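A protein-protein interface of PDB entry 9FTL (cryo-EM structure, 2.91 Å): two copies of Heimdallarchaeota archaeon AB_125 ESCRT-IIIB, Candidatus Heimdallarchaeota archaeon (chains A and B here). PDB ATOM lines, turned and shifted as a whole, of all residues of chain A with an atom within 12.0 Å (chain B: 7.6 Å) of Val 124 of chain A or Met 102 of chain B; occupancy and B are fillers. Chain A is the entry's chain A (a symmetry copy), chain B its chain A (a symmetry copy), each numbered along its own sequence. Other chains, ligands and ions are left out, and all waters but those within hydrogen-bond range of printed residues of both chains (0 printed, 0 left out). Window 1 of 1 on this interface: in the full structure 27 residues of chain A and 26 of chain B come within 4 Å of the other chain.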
ATOM      1  N   THR A 115      39.948  14.568   2.591  1.00  0.00           N
ATOM      2  CA  THR A 115      38.985  15.111   1.638  1.00  0.00           C
ATOM      3  C   THR A 115      38.003  14.040   1.165  1.00  0.00           C
ATOM      4  O   THR A 115      36.786  14.249   1.199  1.00  0.00           O
ATOM      5  CB  THR A 115      39.720  15.736   0.450  1.00  0.00           C
ATOM      6  OG1 THR A 115      40.470  16.870   0.899  1.00  0.00           O
ATOM      7  CG2 THR A 115      38.732  16.198  -0.605  1.00  0.00           C
ATOM      8  N   VAL A 116      38.513  12.892   0.724  1.00  0.00           N
ATOM      9  CA  VAL A 116      37.690  11.780   0.230  1.00  0.00           C
ATOM     10  C   VAL A 116      37.961  10.588   1.140  1.00  0.00           C
ATOM     11  O   VAL A 116      38.907   9.825   0.929  1.00  0.00           O
ATOM     12  CB  VAL A 116      37.982  11.442  -1.234  1.00  0.00           C
ATOM     13  CG1 VAL A 116      37.340  10.115  -1.616  1.00  0.00           C
ATOM     14  CG2 VAL A 116      37.473  12.543  -2.141  1.00  0.00           C
ATOM     15  N   SER A 117      37.118  10.406   2.150  1.00  0.00           N
ATOM     16  CA  SER A 117      37.291   9.307   3.082  1.00  0.00           C
ATOM     17  C   SER A 117      36.789   8.000   2.475  1.00  0.00           C
ATOM     18  O   SER A 117      36.231   7.993   1.378  1.00  0.00           O
ATOM     19  CB  SER A 117      36.545   9.602   4.377  1.00  0.00           C
ATOM     20  OG  SER A 117      35.221  10.026   4.114  1.00  0.00           O
ATOM     21  N   PRO A 118      36.984   6.871   3.165  1.00  0.00           N
ATOM     22  CA  PRO A 118      36.331   5.634   2.704  1.00  0.00           C
ATOM     23  C   PRO A 118      34.830   5.621   2.937  1.00  0.00           C
ATOM     24  O   PRO A 118      34.095   4.958   2.191  1.00  0.00           O
ATOM     25  CB  PRO A 118      37.036   4.552   3.529  1.00  0.00           C
ATOM     26  CG  PRO A 118      38.380   5.103   3.777  1.00  0.00           C
ATOM     27  CD  PRO A 118      38.156   6.572   4.007  1.00  0.00           C
ATOM     28  N   GLU A 119      34.352   6.333   3.960  1.00  0.00           N
ATOM     29  CA  GLU A 119      32.916   6.405   4.206  1.00  0.00           C
ATOM     30  C   GLU A 119      32.197   7.059   3.036  1.00  0.00           C
ATOM     31  O   GLU A 119      31.139   6.589   2.600  1.00  0.00           O
ATOM     32  CB  GLU A 119      32.654   7.172   5.503  1.00  0.00           C
ATOM     33  CG  GLU A 119      31.200   7.146   5.992  1.00  0.00           C
ATOM     34  CD  GLU A 119      30.305   8.212   5.364  1.00  0.00           C
ATOM     35  OE1 GLU A 119      30.819   9.131   4.693  1.00  0.00           O
ATOM     36  OE2 GLU A 119      29.072   8.119   5.538  1.00  0.00           O
ATOM     37  N   ARG A 120      32.760   8.150   2.515  1.00  0.00           N
ATOM     38  CA  ARG A 120      32.175   8.812   1.357  1.00  0.00           C
ATOM     39  C   ARG A 120      32.194   7.896   0.141  1.00  0.00           C
ATOM     40  O   ARG A 120      31.251   7.890  -0.656  1.00  0.00           O
ATOM     41  CB  ARG A 120      32.932  10.113   1.086  1.00  0.00           C
ATOM     42  CG  ARG A 120      32.682  10.758  -0.260  1.00  0.00           C
ATOM     43  CD  ARG A 120      33.215  12.181  -0.264  1.00  0.00           C
ATOM     44  NE  ARG A 120      33.413  12.703  -1.610  1.00  0.00           N
ATOM     45  CZ  ARG A 120      33.732  13.960  -1.893  1.00  0.00           C
ATOM     46  NH1 ARG A 120      33.903  14.866  -0.943  1.00  0.00           N
ATOM     47  NH2 ARG A 120      33.886  14.319  -3.164  1.00  0.00           N
ATOM     48  N   THR A 121      33.251   7.095  -0.003  1.00  0.00           N
ATOM     49  CA  THR A 121      33.319   6.157  -1.118  1.00  0.00           C
ATOM     50  C   THR A 121      32.221   5.107  -1.022  1.00  0.00           C
ATOM     51  O   THR A 121      31.566   4.783  -2.024  1.00  0.00           O
ATOM     52  CB  THR A 121      34.693   5.486  -1.147  1.00  0.00           C
ATOM     53  OG1 THR A 121      35.701   6.474  -1.382  1.00  0.00           O
ATOM     54  CG2 THR A 121      34.761   4.436  -2.240  1.00  0.00           C
ATOM     55  N   GLU A 122      31.990   4.571   0.176  1.00  0.00           N
ATOM     56  CA  GLU A 122      30.965   3.546   0.320  1.00  0.00           C
ATOM     57  C   GLU A 122      29.576   4.140   0.142  1.00  0.00           C
ATOM     58  O   GLU A 122      28.686   3.495  -0.421  1.00  0.00           O
ATOM     59  CB  GLU A 122      31.093   2.862   1.680  1.00  0.00           C
ATOM     60  CG  GLU A 122      32.368   2.049   1.848  1.00  0.00           C
ATOM     61  CD  GLU A 122      32.328   0.714   1.125  1.00  0.00           C
ATOM     62  OE1 GLU A 122      33.133  -0.173   1.476  1.00  0.00           O
ATOM     63  OE2 GLU A 122      31.488   0.540   0.218  1.00  0.00           O
ATOM     64  N   ARG A 123      29.377   5.377   0.597  1.00  0.00           N
ATOM     65  CA  ARG A 123      28.107   6.052   0.360  1.00  0.00           C
ATOM     66  C   ARG A 123      27.863   6.254  -1.132  1.00  0.00           C
ATOM     67  O   ARG A 123      26.747   6.039  -1.624  1.00  0.00           O
ATOM     68  CB  ARG A 123      28.098   7.387   1.105  1.00  0.00           C
ATOM     69  CG  ARG A 123      27.092   8.407   0.602  1.00  0.00           C
ATOM     70  CD  ARG A 123      26.768   9.441   1.669  1.00  0.00           C
ATOM     71  NE  ARG A 123      27.930   9.784   2.484  1.00  0.00           N
ATOM     72  CZ  ARG A 123      28.802  10.750   2.221  1.00  0.00           C
ATOM     73  NH1 ARG A 123      28.712  11.498   1.130  1.00  0.00           N
ATOM     74  NH2 ARG A 123      29.801  10.967   3.071  1.00  0.00           N
ATOM     75  N   VAL A 124      28.903   6.649  -1.870  1.00  0.00           N
ATOM     76  CA  VAL A 124      28.760   6.861  -3.307  1.00  0.00           C
ATOM     77  C   VAL A 124      28.409   5.554  -4.004  1.00  0.00           C
ATOM     78  O   VAL A 124      27.517   5.511  -4.859  1.00  0.00           O
ATOM     79  CB  VAL A 124      30.047   7.487  -3.879  1.00  0.00           C
ATOM     80  CG1 VAL A 124      30.118   7.345  -5.391  1.00  0.00           C
ATOM     81  CG2 VAL A 124      30.136   8.948  -3.488  1.00  0.00           C
ATOM     82  N   MET A 125      29.095   4.467  -3.655  1.00  0.00           N
ATOM     83  CA  MET A 125      28.793   3.197  -4.302  1.00  0.00           C
ATOM     84  C   MET A 125      27.422   2.655  -3.916  1.00  0.00           C
ATOM     85  O   MET A 125      26.755   2.039  -4.755  1.00  0.00           O
ATOM     86  CB  MET A 125      29.871   2.165  -3.977  1.00  0.00           C
ATOM     87  CG  MET A 125      31.262   2.535  -4.481  1.00  0.00           C
ATOM     88  SD  MET A 125      31.388   2.743  -6.272  1.00  0.00           S
ATOM     89  CE  MET A 125      30.998   1.095  -6.852  1.00  0.00           C
ATOM     90  N   ASP A 126      26.968   2.897  -2.686  1.00  0.00           N
ATOM     91  CA  ASP A 126      25.610   2.514  -2.325  1.00  0.00           C
ATOM     92  C   ASP A 126      24.590   3.287  -3.148  1.00  0.00           C
ATOM     93  O   ASP A 126      23.586   2.722  -3.593  1.00  0.00           O
ATOM     94  CB  ASP A 126      25.375   2.748  -0.834  1.00  0.00           C
ATOM     95  CG  ASP A 126      26.122   1.759   0.039  1.00  0.00           C
ATOM     96  OD1 ASP A 126      26.753   0.829  -0.505  1.00  0.00           O
ATOM     97  OD2 ASP A 126      26.077   1.912   1.276  1.00  0.00           O
ATOM     98  N   SER A 127      24.835   4.582  -3.363  1.00  0.00           N
ATOM     99  CA  SER A 127      23.939   5.361  -4.212  1.00  0.00           C
ATOM    100  C   SER A 127      23.934   4.841  -5.642  1.00  0.00           C
ATOM    101  O   SER A 127      22.876   4.789  -6.279  1.00  0.00           O
ATOM    102  CB  SER A 127      24.338   6.833  -4.194  1.00  0.00           C
ATOM    103  OG  SER A 127      25.625   7.010  -4.754  1.00  0.00           O
ATOM    104  N   VAL A 128      25.099   4.447  -6.155  1.00  0.00           N
ATOM    105  CA  VAL A 128      25.171   3.898  -7.505  1.00  0.00           C
ATOM    106  C   VAL A 128      24.340   2.625  -7.610  1.00  0.00           C
ATOM    107  O   VAL A 128      23.577   2.446  -8.566  1.00  0.00           O
ATOM    108  CB  VAL A 128      26.638   3.651  -7.904  1.00  0.00           C
ATOM    109  CG1 VAL A 128      26.726   2.843  -9.184  1.00  0.00           C
ATOM    110  CG2 VAL A 128      27.371   4.964  -8.078  1.00  0.00           C
ATOM    111  N   MET A 129      24.457   1.730  -6.629  1.00  0.00           N
ATOM    112  CA  MET A 129      23.712   0.475  -6.700  1.00  0.00           C
ATOM    113  C   MET A 129      22.211   0.706  -6.542  1.00  0.00           C
ATOM    114  O   MET A 129      21.402   0.065  -7.225  1.00  0.00           O
ATOM    115  CB  MET A 129      24.224  -0.506  -5.644  1.00  0.00           C
ATOM    116  CG  MET A 129      25.705  -0.854  -5.776  1.00  0.00           C
ATOM    117  SD  MET A 129      26.108  -1.904  -7.176  1.00  0.00           S
ATOM    118  CE  MET A 129      26.376  -3.471  -6.353  1.00  0.00           C
ATOM    119  N   GLU A 130      21.816   1.628  -5.659  1.00  0.00           N
ATOM    120  CA  GLU A 130      20.397   1.930  -5.502  1.00  0.00           C
ATOM    121  C   GLU A 130      19.805   2.516  -6.778  1.00  0.00           C
ATOM    122  O   GLU A 130      18.695   2.146  -7.186  1.00  0.00           O
ATOM    123  CB  GLU A 130      20.198   2.897  -4.331  1.00  0.00           C
ATOM    124  CG  GLU A 130      18.753   3.127  -3.819  1.00  0.00           C
ATOM    125  CD  GLU A 130      17.797   1.949  -3.992  1.00  0.00           C
ATOM    126  OE1 GLU A 130      18.172   0.806  -3.656  1.00  0.00           O
ATOM    127  OE2 GLU A 130      16.661   2.169  -4.463  1.00  0.00           O
ATOM    128  N   GLN A 131      20.531   3.426  -7.430  1.00  0.00           N
ATOM    129  CA  GLN A 131      20.018   4.001  -8.666  1.00  0.00           C
ATOM    130  C   GLN A 131      19.998   2.975  -9.788  1.00  0.00           C
ATOM    131  O   GLN A 131      19.118   3.025 -10.651  1.00  0.00           O
ATOM    132  CB  GLN A 131      20.844   5.218  -9.062  1.00  0.00           C
ATOM    133  CG  GLN A 131      20.622   6.412  -8.160  1.00  0.00           C
ATOM    134  CD  GLN A 131      21.594   7.531  -8.432  1.00  0.00           C
ATOM    135  OE1 GLN A 131      22.519   7.383  -9.227  1.00  0.00           O
ATOM    136  NE2 GLN A 131      21.395   8.661  -7.769  1.00  0.00           N
ATOM    137  N   ARG A 132      20.942   2.033  -9.792  1.00  0.00           N
ATOM    138  CA  ARG A 132      20.875   0.943 -10.758  1.00  0.00           C
ATOM    139  C   ARG A 132      19.621   0.102 -10.549  1.00  0.00           C
ATOM    140  O   ARG A 132      18.944  -0.266 -11.516  1.00  0.00           O
ATOM    141  CB  ARG A 132      22.125   0.074 -10.650  1.00  0.00           C
ATOM    142  CG  ARG A 132      22.529  -0.597 -11.945  1.00  0.00           C
ATOM    143  CD  ARG A 132      23.782  -1.434 -11.764  1.00  0.00           C
ATOM    144  NE  ARG A 132      24.945  -0.629 -11.413  1.00  0.00           N
ATOM    145  CZ  ARG A 132      26.170  -1.105 -11.225  1.00  0.00           C
ATOM    146  NH1 ARG A 132      26.440  -2.396 -11.330  1.00  0.00           N
ATOM    147  NH2 ARG A 132      27.151  -0.262 -10.918  1.00  0.00           N
ATOM    148  N   ASP A 133      19.283  -0.191  -9.290  1.00  0.00           N
ATOM    149  CA  ASP A 133      18.054  -0.931  -9.005  1.00  0.00           C
ATOM    150  C   ASP A 133      16.825  -0.175  -9.492  1.00  0.00           C
ATOM    151  O   ASP A 133      15.921  -0.763 -10.100  1.00  0.00           O
ATOM    152  CB  ASP A 133      17.935  -1.189  -7.502  1.00  0.00           C
ATOM    153  CG  ASP A 133      18.814  -2.324  -7.024  1.00  0.00           C
ATOM    154  OD1 ASP A 133      19.082  -3.254  -7.805  1.00  0.00           O
ATOM    155  OD2 ASP A 133      19.233  -2.285  -5.852  1.00  0.00           O
ATOM    156  N   GLN A 134      16.767   1.128  -9.223  1.00  0.00           N
ATOM    157  CA  GLN A 134      15.602   1.909  -9.630  1.00  0.00           C
ATOM    158  C   GLN A 134      15.481   1.983 -11.149  1.00  0.00           C
ATOM    159  O   GLN A 134      14.375   1.873 -11.699  1.00  0.00           O
ATOM    160  CB  GLN A 134      15.678   3.306  -9.025  1.00  0.00           C
ATOM    161  CG  GLN A 134      15.230   3.356  -7.580  1.00  0.00           C
ATOM    162  CD  GLN A 134      15.439   4.709  -6.950  1.00  0.00           C
ATOM    163  OE1 GLN A 134      16.242   5.508  -7.423  1.00  0.00           O
ATOM    164  NE2 GLN A 134      14.715   4.978  -5.871  1.00  0.00           N
ATOM    165  N   ILE A 135      16.602   2.172 -11.845  1.00  0.00           N
ATOM    166  CA  ILE A 135      16.565   2.231 -13.301  1.00  0.00           C
ATOM    167  C   ILE A 135      16.139   0.887 -13.871  1.00  0.00           C
ATOM    168  O   ILE A 135      15.417   0.828 -14.871  1.00  0.00           O
ATOM    169  CB  ILE A 135      17.931   2.682 -13.853  1.00  0.00           C
ATOM    170  CG1 ILE A 135      18.130   4.175 -13.610  1.00  0.00           C
ATOM    171  CG2 ILE A 135      18.049   2.398 -15.346  1.00  0.00           C
ATOM    172  CD1 ILE A 135      19.574   4.590 -13.538  1.00  0.00           C
ATOM    173  N   THR B  95      42.207   8.349  -7.046  1.00  0.00           N
ATOM    174  CA  THR B  95      41.014   7.835  -6.386  1.00  0.00           C
ATOM    175  C   THR B  95      40.066   8.964  -6.002  1.00  0.00           C
ATOM    176  O   THR B  95      38.845   8.826  -6.142  1.00  0.00           O
ATOM    177  CB  THR B  95      41.414   7.020  -5.158  1.00  0.00           C
ATOM    178  OG1 THR B  95      42.031   5.799  -5.578  1.00  0.00           O
ATOM    179  CG2 THR B  95      40.201   6.686  -4.303  1.00  0.00           C
ATOM    180  N   ALA B  96      40.600  10.084  -5.510  1.00  0.00           N
ATOM    181  CA  ALA B  96      39.731  11.206  -5.173  1.00  0.00           C
ATOM    182  C   ALA B  96      39.021  11.744  -6.410  1.00  0.00           C
ATOM    183  O   ALA B  96      37.816  12.037  -6.367  1.00  0.00           O
ATOM    184  CB  ALA B  96      40.538  12.306  -4.491  1.00  0.00           C
ATOM    185  N   GLU B  97      39.742  11.860  -7.529  1.00  0.00           N
ATOM    186  CA  GLU B  97      39.103  12.349  -8.749  1.00  0.00           C
ATOM    187  C   GLU B  97      38.023  11.389  -9.236  1.00  0.00           C
ATOM    188  O   GLU B  97      36.945  11.818  -9.675  1.00  0.00           O
ATOM    189  CB  GLU B  97      40.153  12.574  -9.834  1.00  0.00           C
ATOM    190  CG  GLU B  97      40.766  13.969  -9.797  1.00  0.00           C
ATOM    191  CD  GLU B  97      42.239  13.994 -10.154  1.00  0.00           C
ATOM    192  OE1 GLU B  97      42.718  13.059 -10.831  1.00  0.00           O
ATOM    193  OE2 GLU B  97      42.927  14.958  -9.755  1.00  0.00           O
ATOM    194  N   THR B  98      38.291  10.082  -9.163  1.00  0.00           N
ATOM    195  CA  THR B  98      37.299   9.097  -9.579  1.00  0.00           C
ATOM    196  C   THR B  98      36.051   9.167  -8.709  1.00  0.00           C
ATOM    197  O   THR B  98      34.926   9.080  -9.217  1.00  0.00           O
ATOM    198  CB  THR B  98      37.903   7.696  -9.530  1.00  0.00           C
ATOM    199  OG1 THR B  98      38.978   7.608 -10.472  1.00  0.00           O
ATOM    200  CG2 THR B  98      36.863   6.648  -9.868  1.00  0.00           C
ATOM    201  N   VAL B  99      36.228   9.324  -7.398  1.00  0.00           N
ATOM    202  CA  VAL B  99      35.073   9.402  -6.513  1.00  0.00           C
ATOM    203  C   VAL B  99      34.263  10.657  -6.807  1.00  0.00           C
ATOM    204  O   VAL B  99      33.028  10.630  -6.751  1.00  0.00           O
ATOM    205  CB  VAL B  99      35.529   9.340  -5.043  1.00  0.00           C
ATOM    206  CG1 VAL B  99      34.418   9.779  -4.099  1.00  0.00           C
ATOM    207  CG2 VAL B  99      35.993   7.940  -4.699  1.00  0.00           C
ATOM    208  N   LYS B 100      34.925  11.767  -7.136  1.00  0.00           N
ATOM    209  CA  LYS B 100      34.175  12.977  -7.465  1.00  0.00           C
ATOM    210  C   LYS B 100      33.378  12.807  -8.755  1.00  0.00           C
ATOM    211  O   LYS B 100      32.226  13.255  -8.848  1.00  0.00           O
ATOM    212  CB  LYS B 100      35.122  14.169  -7.576  1.00  0.00           C
ATOM    213  CG  LYS B 100      35.860  14.479  -6.293  1.00  0.00           C
ATOM    214  CD  LYS B 100      35.660  15.924  -5.868  1.00  0.00           C
ATOM    215  CE  LYS B 100      36.547  16.303  -4.693  1.00  0.00           C
ATOM    216  NZ  LYS B 100      37.997  16.217  -5.011  1.00  0.00           N
ATOM    217  N   ALA B 101      33.968  12.155  -9.760  1.00  0.00           N
ATOM    218  CA  ALA B 101      33.227  11.890 -10.992  1.00  0.00           C
ATOM    219  C   ALA B 101      32.015  11.000 -10.732  1.00  0.00           C
ATOM    220  O   ALA B 101      30.916  11.263 -11.247  1.00  0.00           O
ATOM    221  CB  ALA B 101      34.148  11.248 -12.026  1.00  0.00           C
ATOM    222  N   MET B 102      32.197   9.936  -9.945  1.00  0.00           N
ATOM    223  CA  MET B 102      31.079   9.052  -9.631  1.00  0.00           C
ATOM    224  C   MET B 102      29.981   9.795  -8.881  1.00  0.00           C
ATOM    225  O   MET B 102      28.792   9.568  -9.129  1.00  0.00           O
ATOM    226  CB  MET B 102      31.561   7.858  -8.811  1.00  0.00           C
ATOM    227  CG  MET B 102      32.093   6.713  -9.641  1.00  0.00           C
ATOM    228  SD  MET B 102      33.204   5.648  -8.710  1.00  0.00           S
ATOM    229  CE  MET B 102      33.422   4.294  -9.857  1.00  0.00           C
ATOM    230  N   GLU B 103      30.357  10.681  -7.960  1.00  0.00           N
ATOM    231  CA  GLU B 103      29.360  11.467  -7.243  1.00  0.00           C
ATOM    232  C   GLU B 103      28.593  12.389  -8.180  1.00  0.00           C
ATOM    233  O   GLU B 103      27.380  12.567  -8.017  1.00  0.00           O
ATOM    234  CB  GLU B 103      30.035  12.275  -6.137  1.00  0.00           C
ATOM    235  CG  GLU B 103      29.160  12.570  -4.928  1.00  0.00           C
ATOM    236  CD  GLU B 103      29.970  12.804  -3.669  1.00  0.00           C
ATOM    237  OE1 GLU B 103      31.163  13.153  -3.779  1.00  0.00           O
ATOM    238  OE2 GLU B 103      29.414  12.640  -2.563  1.00  0.00           O
ATOM    239  N   LEU B 104      29.273  12.977  -9.167  1.00  0.00           N
ATOM    240  CA  LEU B 104      28.578  13.815 -10.142  1.00  0.00           C
ATOM    241  C   LEU B 104      27.552  13.004 -10.929  1.00  0.00           C
ATOM    242  O   LEU B 104      26.398  13.428 -11.100  1.00  0.00           O
ATOM    243  CB  LEU B 104      29.593  14.454 -11.090  1.00  0.00           C
ATOM    244  CG  LEU B 104      29.162  15.653 -11.938  1.00  0.00           C
ATOM    245  CD1 LEU B 104      28.627  16.796 -11.087  1.00  0.00           C
ATOM    246  CD2 LEU B 104      30.329  16.121 -12.788  1.00  0.00           C
ATOM    247  N   GLY B 105      27.963  11.835 -11.419  1.00  0.00           N
ATOM    248  CA  GLY B 105      27.030  10.986 -12.146  1.00  0.00           C
ATOM    249  C   GLY B 105      25.851  10.560 -11.293  1.00  0.00           C
ATOM    250  O   GLY B 105      24.713  10.503 -11.767  1.00  0.00           O
ATOM    251  N   THR B 106      26.110  10.251 -10.020  1.00  0.00           N
ATOM    252  CA  THR B 106      25.037   9.865  -9.112  1.00  0.00           C
ATOM    253  C   THR B 106      24.059  11.015  -8.914  1.00  0.00           C
ATOM    254  O   THR B 106      22.847  10.798  -8.854  1.00  0.00           O
ATOM    255  CB  THR B 106      25.634   9.392  -7.778  1.00  0.00           C
ATOM    256  OG1 THR B 106      26.411  10.452  -7.210  1.00  0.00           O
ATOM    257  CG2 THR B 106      26.538   8.159  -7.927  1.00  0.00           C
ATOM    258  N   LYS B 107      24.566  12.245  -8.807  1.00  0.00           N
ATOM    259  CA  LYS B 107      23.678  13.398  -8.679  1.00  0.00           C
ATOM    260  C   LYS B 107      22.787  13.549  -9.906  1.00  0.00           C
ATOM    261  O   LYS B 107      21.576  13.792  -9.784  1.00  0.00           O
ATOM    262  CB  LYS B 107      24.506  14.664  -8.470  1.00  0.00           C
ATOM    263  CG  LYS B 107      23.707  15.859  -7.966  1.00  0.00           C
ATOM    264  CD  LYS B 107      24.591  16.961  -7.367  1.00  0.00           C
ATOM    265  CE  LYS B 107      25.316  16.560  -6.077  1.00  0.00           C
ATOM    266  NZ  LYS B 107      24.467  15.820  -5.103  1.00  0.00           N
ATOM    267  N   VAL B 108      23.367  13.391 -11.099  1.00  0.00           N
ATOM    268  CA  VAL B 108      22.585  13.538 -12.327  1.00  0.00           C
ATOM    269  C   VAL B 108      21.491  12.476 -12.391  1.00  0.00           C
ATOM    270  O   VAL B 108      20.318  12.775 -12.664  1.00  0.00           O
ATOM    271  CB  VAL B 108      23.513  13.479 -13.557  1.00  0.00           C
ATOM    272  CG1 VAL B 108      22.741  13.155 -14.839  1.00  0.00           C
ATOM    273  CG2 VAL B 108      24.260  14.787 -13.700  1.00  0.00           C
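The side-chain amide nitrogen (NE2) of Gln 131 of chain A sits at hydrogen-bond distance from the backbone carbonyl oxygen (O) of Thr 106 of chain B (2.8 Å). The guanidinium group of Arg 123 of chain A lies within salt-bridge range of the side-chain carboxylate of Glu 103 of chain B, 3.9 Å away. NH2 of Arg 120 of chain A is in salt-bridge range of OE1 of Glu 103 of chain B, 3.0 Å away.
The backbone carbonyl oxygen (O) of Met 102 of chain B lies close to the side-chain hydroxyl (OG1) of Thr 106 of chain B, 3.2 Å away. The side-chain hydroxyl (OG) of Ser 127 of chain A sits at hydrogen-bond distance from the backbone carbonyl oxygen (O) of Val 124 of chain A (2.4 Å). O of Arg 123 of chain A lies within hydrogen-bond range of OG of Ser 127 of chain A (3.5 Å). The side-chain hydroxyl of Thr 121 of chain A is in hydrogen-bond range of the backbone carbonyl oxygen of Ser 117 of chain A, at 3.2 Å. The backbone carbonyl oxygen (O) of Glu 103 of chain B sits at hydrogen-bond distance from the side-chain hydroxyl (OG1) of Thr 106 of chain B (2.5 Å). N of Arg 120 of chain A sits at hydrogen-bond distance from OG of Ser 117 of chain A.
Val 116 of chain A touches Ala 96 of chain B (CG2 to CB, 3.9 Å). Val 99 of chain B touches Val 116 of chain A (CG1 to CG1, 3.8 Å). Val 99 of chain B touches Arg 120 of chain A. NH2 of Arg 120 of chain A touches CD of Lys 100 of chain B, at 3.6 Å. CG2 of Val 99 of chain B touches OG1 of Thr 121 of chain A, 3.6 Å away. CG1 of Val 124 of chain A touches CB of Met 102 of chain B (3.7 Å). CG2 of Val 124 of chain A touches CD of Glu 103 of chain B, at 3.9 Å. Ser 127 of chain A touches Thr 106 of chain B. Val 128 of chain A touches Thr 106 of chain B.
Of the printed residues of chain B, Thr 121 of chain A touches Val 99. Val 124 of chain A touches just these residues of chain B: Met 102 and Glu 103. Printed residues of chain B within 4 Å of Ser 127 of chain A: Thr 106 (3.5 Å). Arg 132 of chain A touches none of the printed residues of chain B. No residue of chain A comes within 4 Å of Thr 98 of chain B. Printed residues of chain A within 4 Å of Val 99 of chain B: Val 116, Arg 120 and Thr 121. Printed residues of chain A within 4 Å of Lys 100 of chain B: Arg 120. No residue of chain A comes within 4 Å of Ala 101 of chain B. Printed residues of chain A within 4 Å of Met 102 of chain B: Val 124 (3.7 Å). Glu 103 of chain B touches just these residues of chain A: Arg 120 (3.0 Å), Arg 123 (3.9 Å) and Val 124 (3.9 Å). No residue of chain A comes within 4 Å of Leu 104 of chain B. No residue of chain A comes within 4 Å of Gly 105 of chain B. Thr 106 of chain B touches just these residues of chain A: Ser 127, Val 128 and Gln 131.
Of the 14 printed residues of chain B, 6 touch a printed residue of chain A. Hydrophobic or aromatic side chains of chain B within 4 Å of the printed part of chain A: Ala 96, Val 99 and Met 102. Hydrophobic or aromatic side chains of chain A that line the printed part of chain B: Val 116, Val 124 and Val 128. Among the printed residues, 12 pairs touch across the chains.
No position is printed for both chains.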
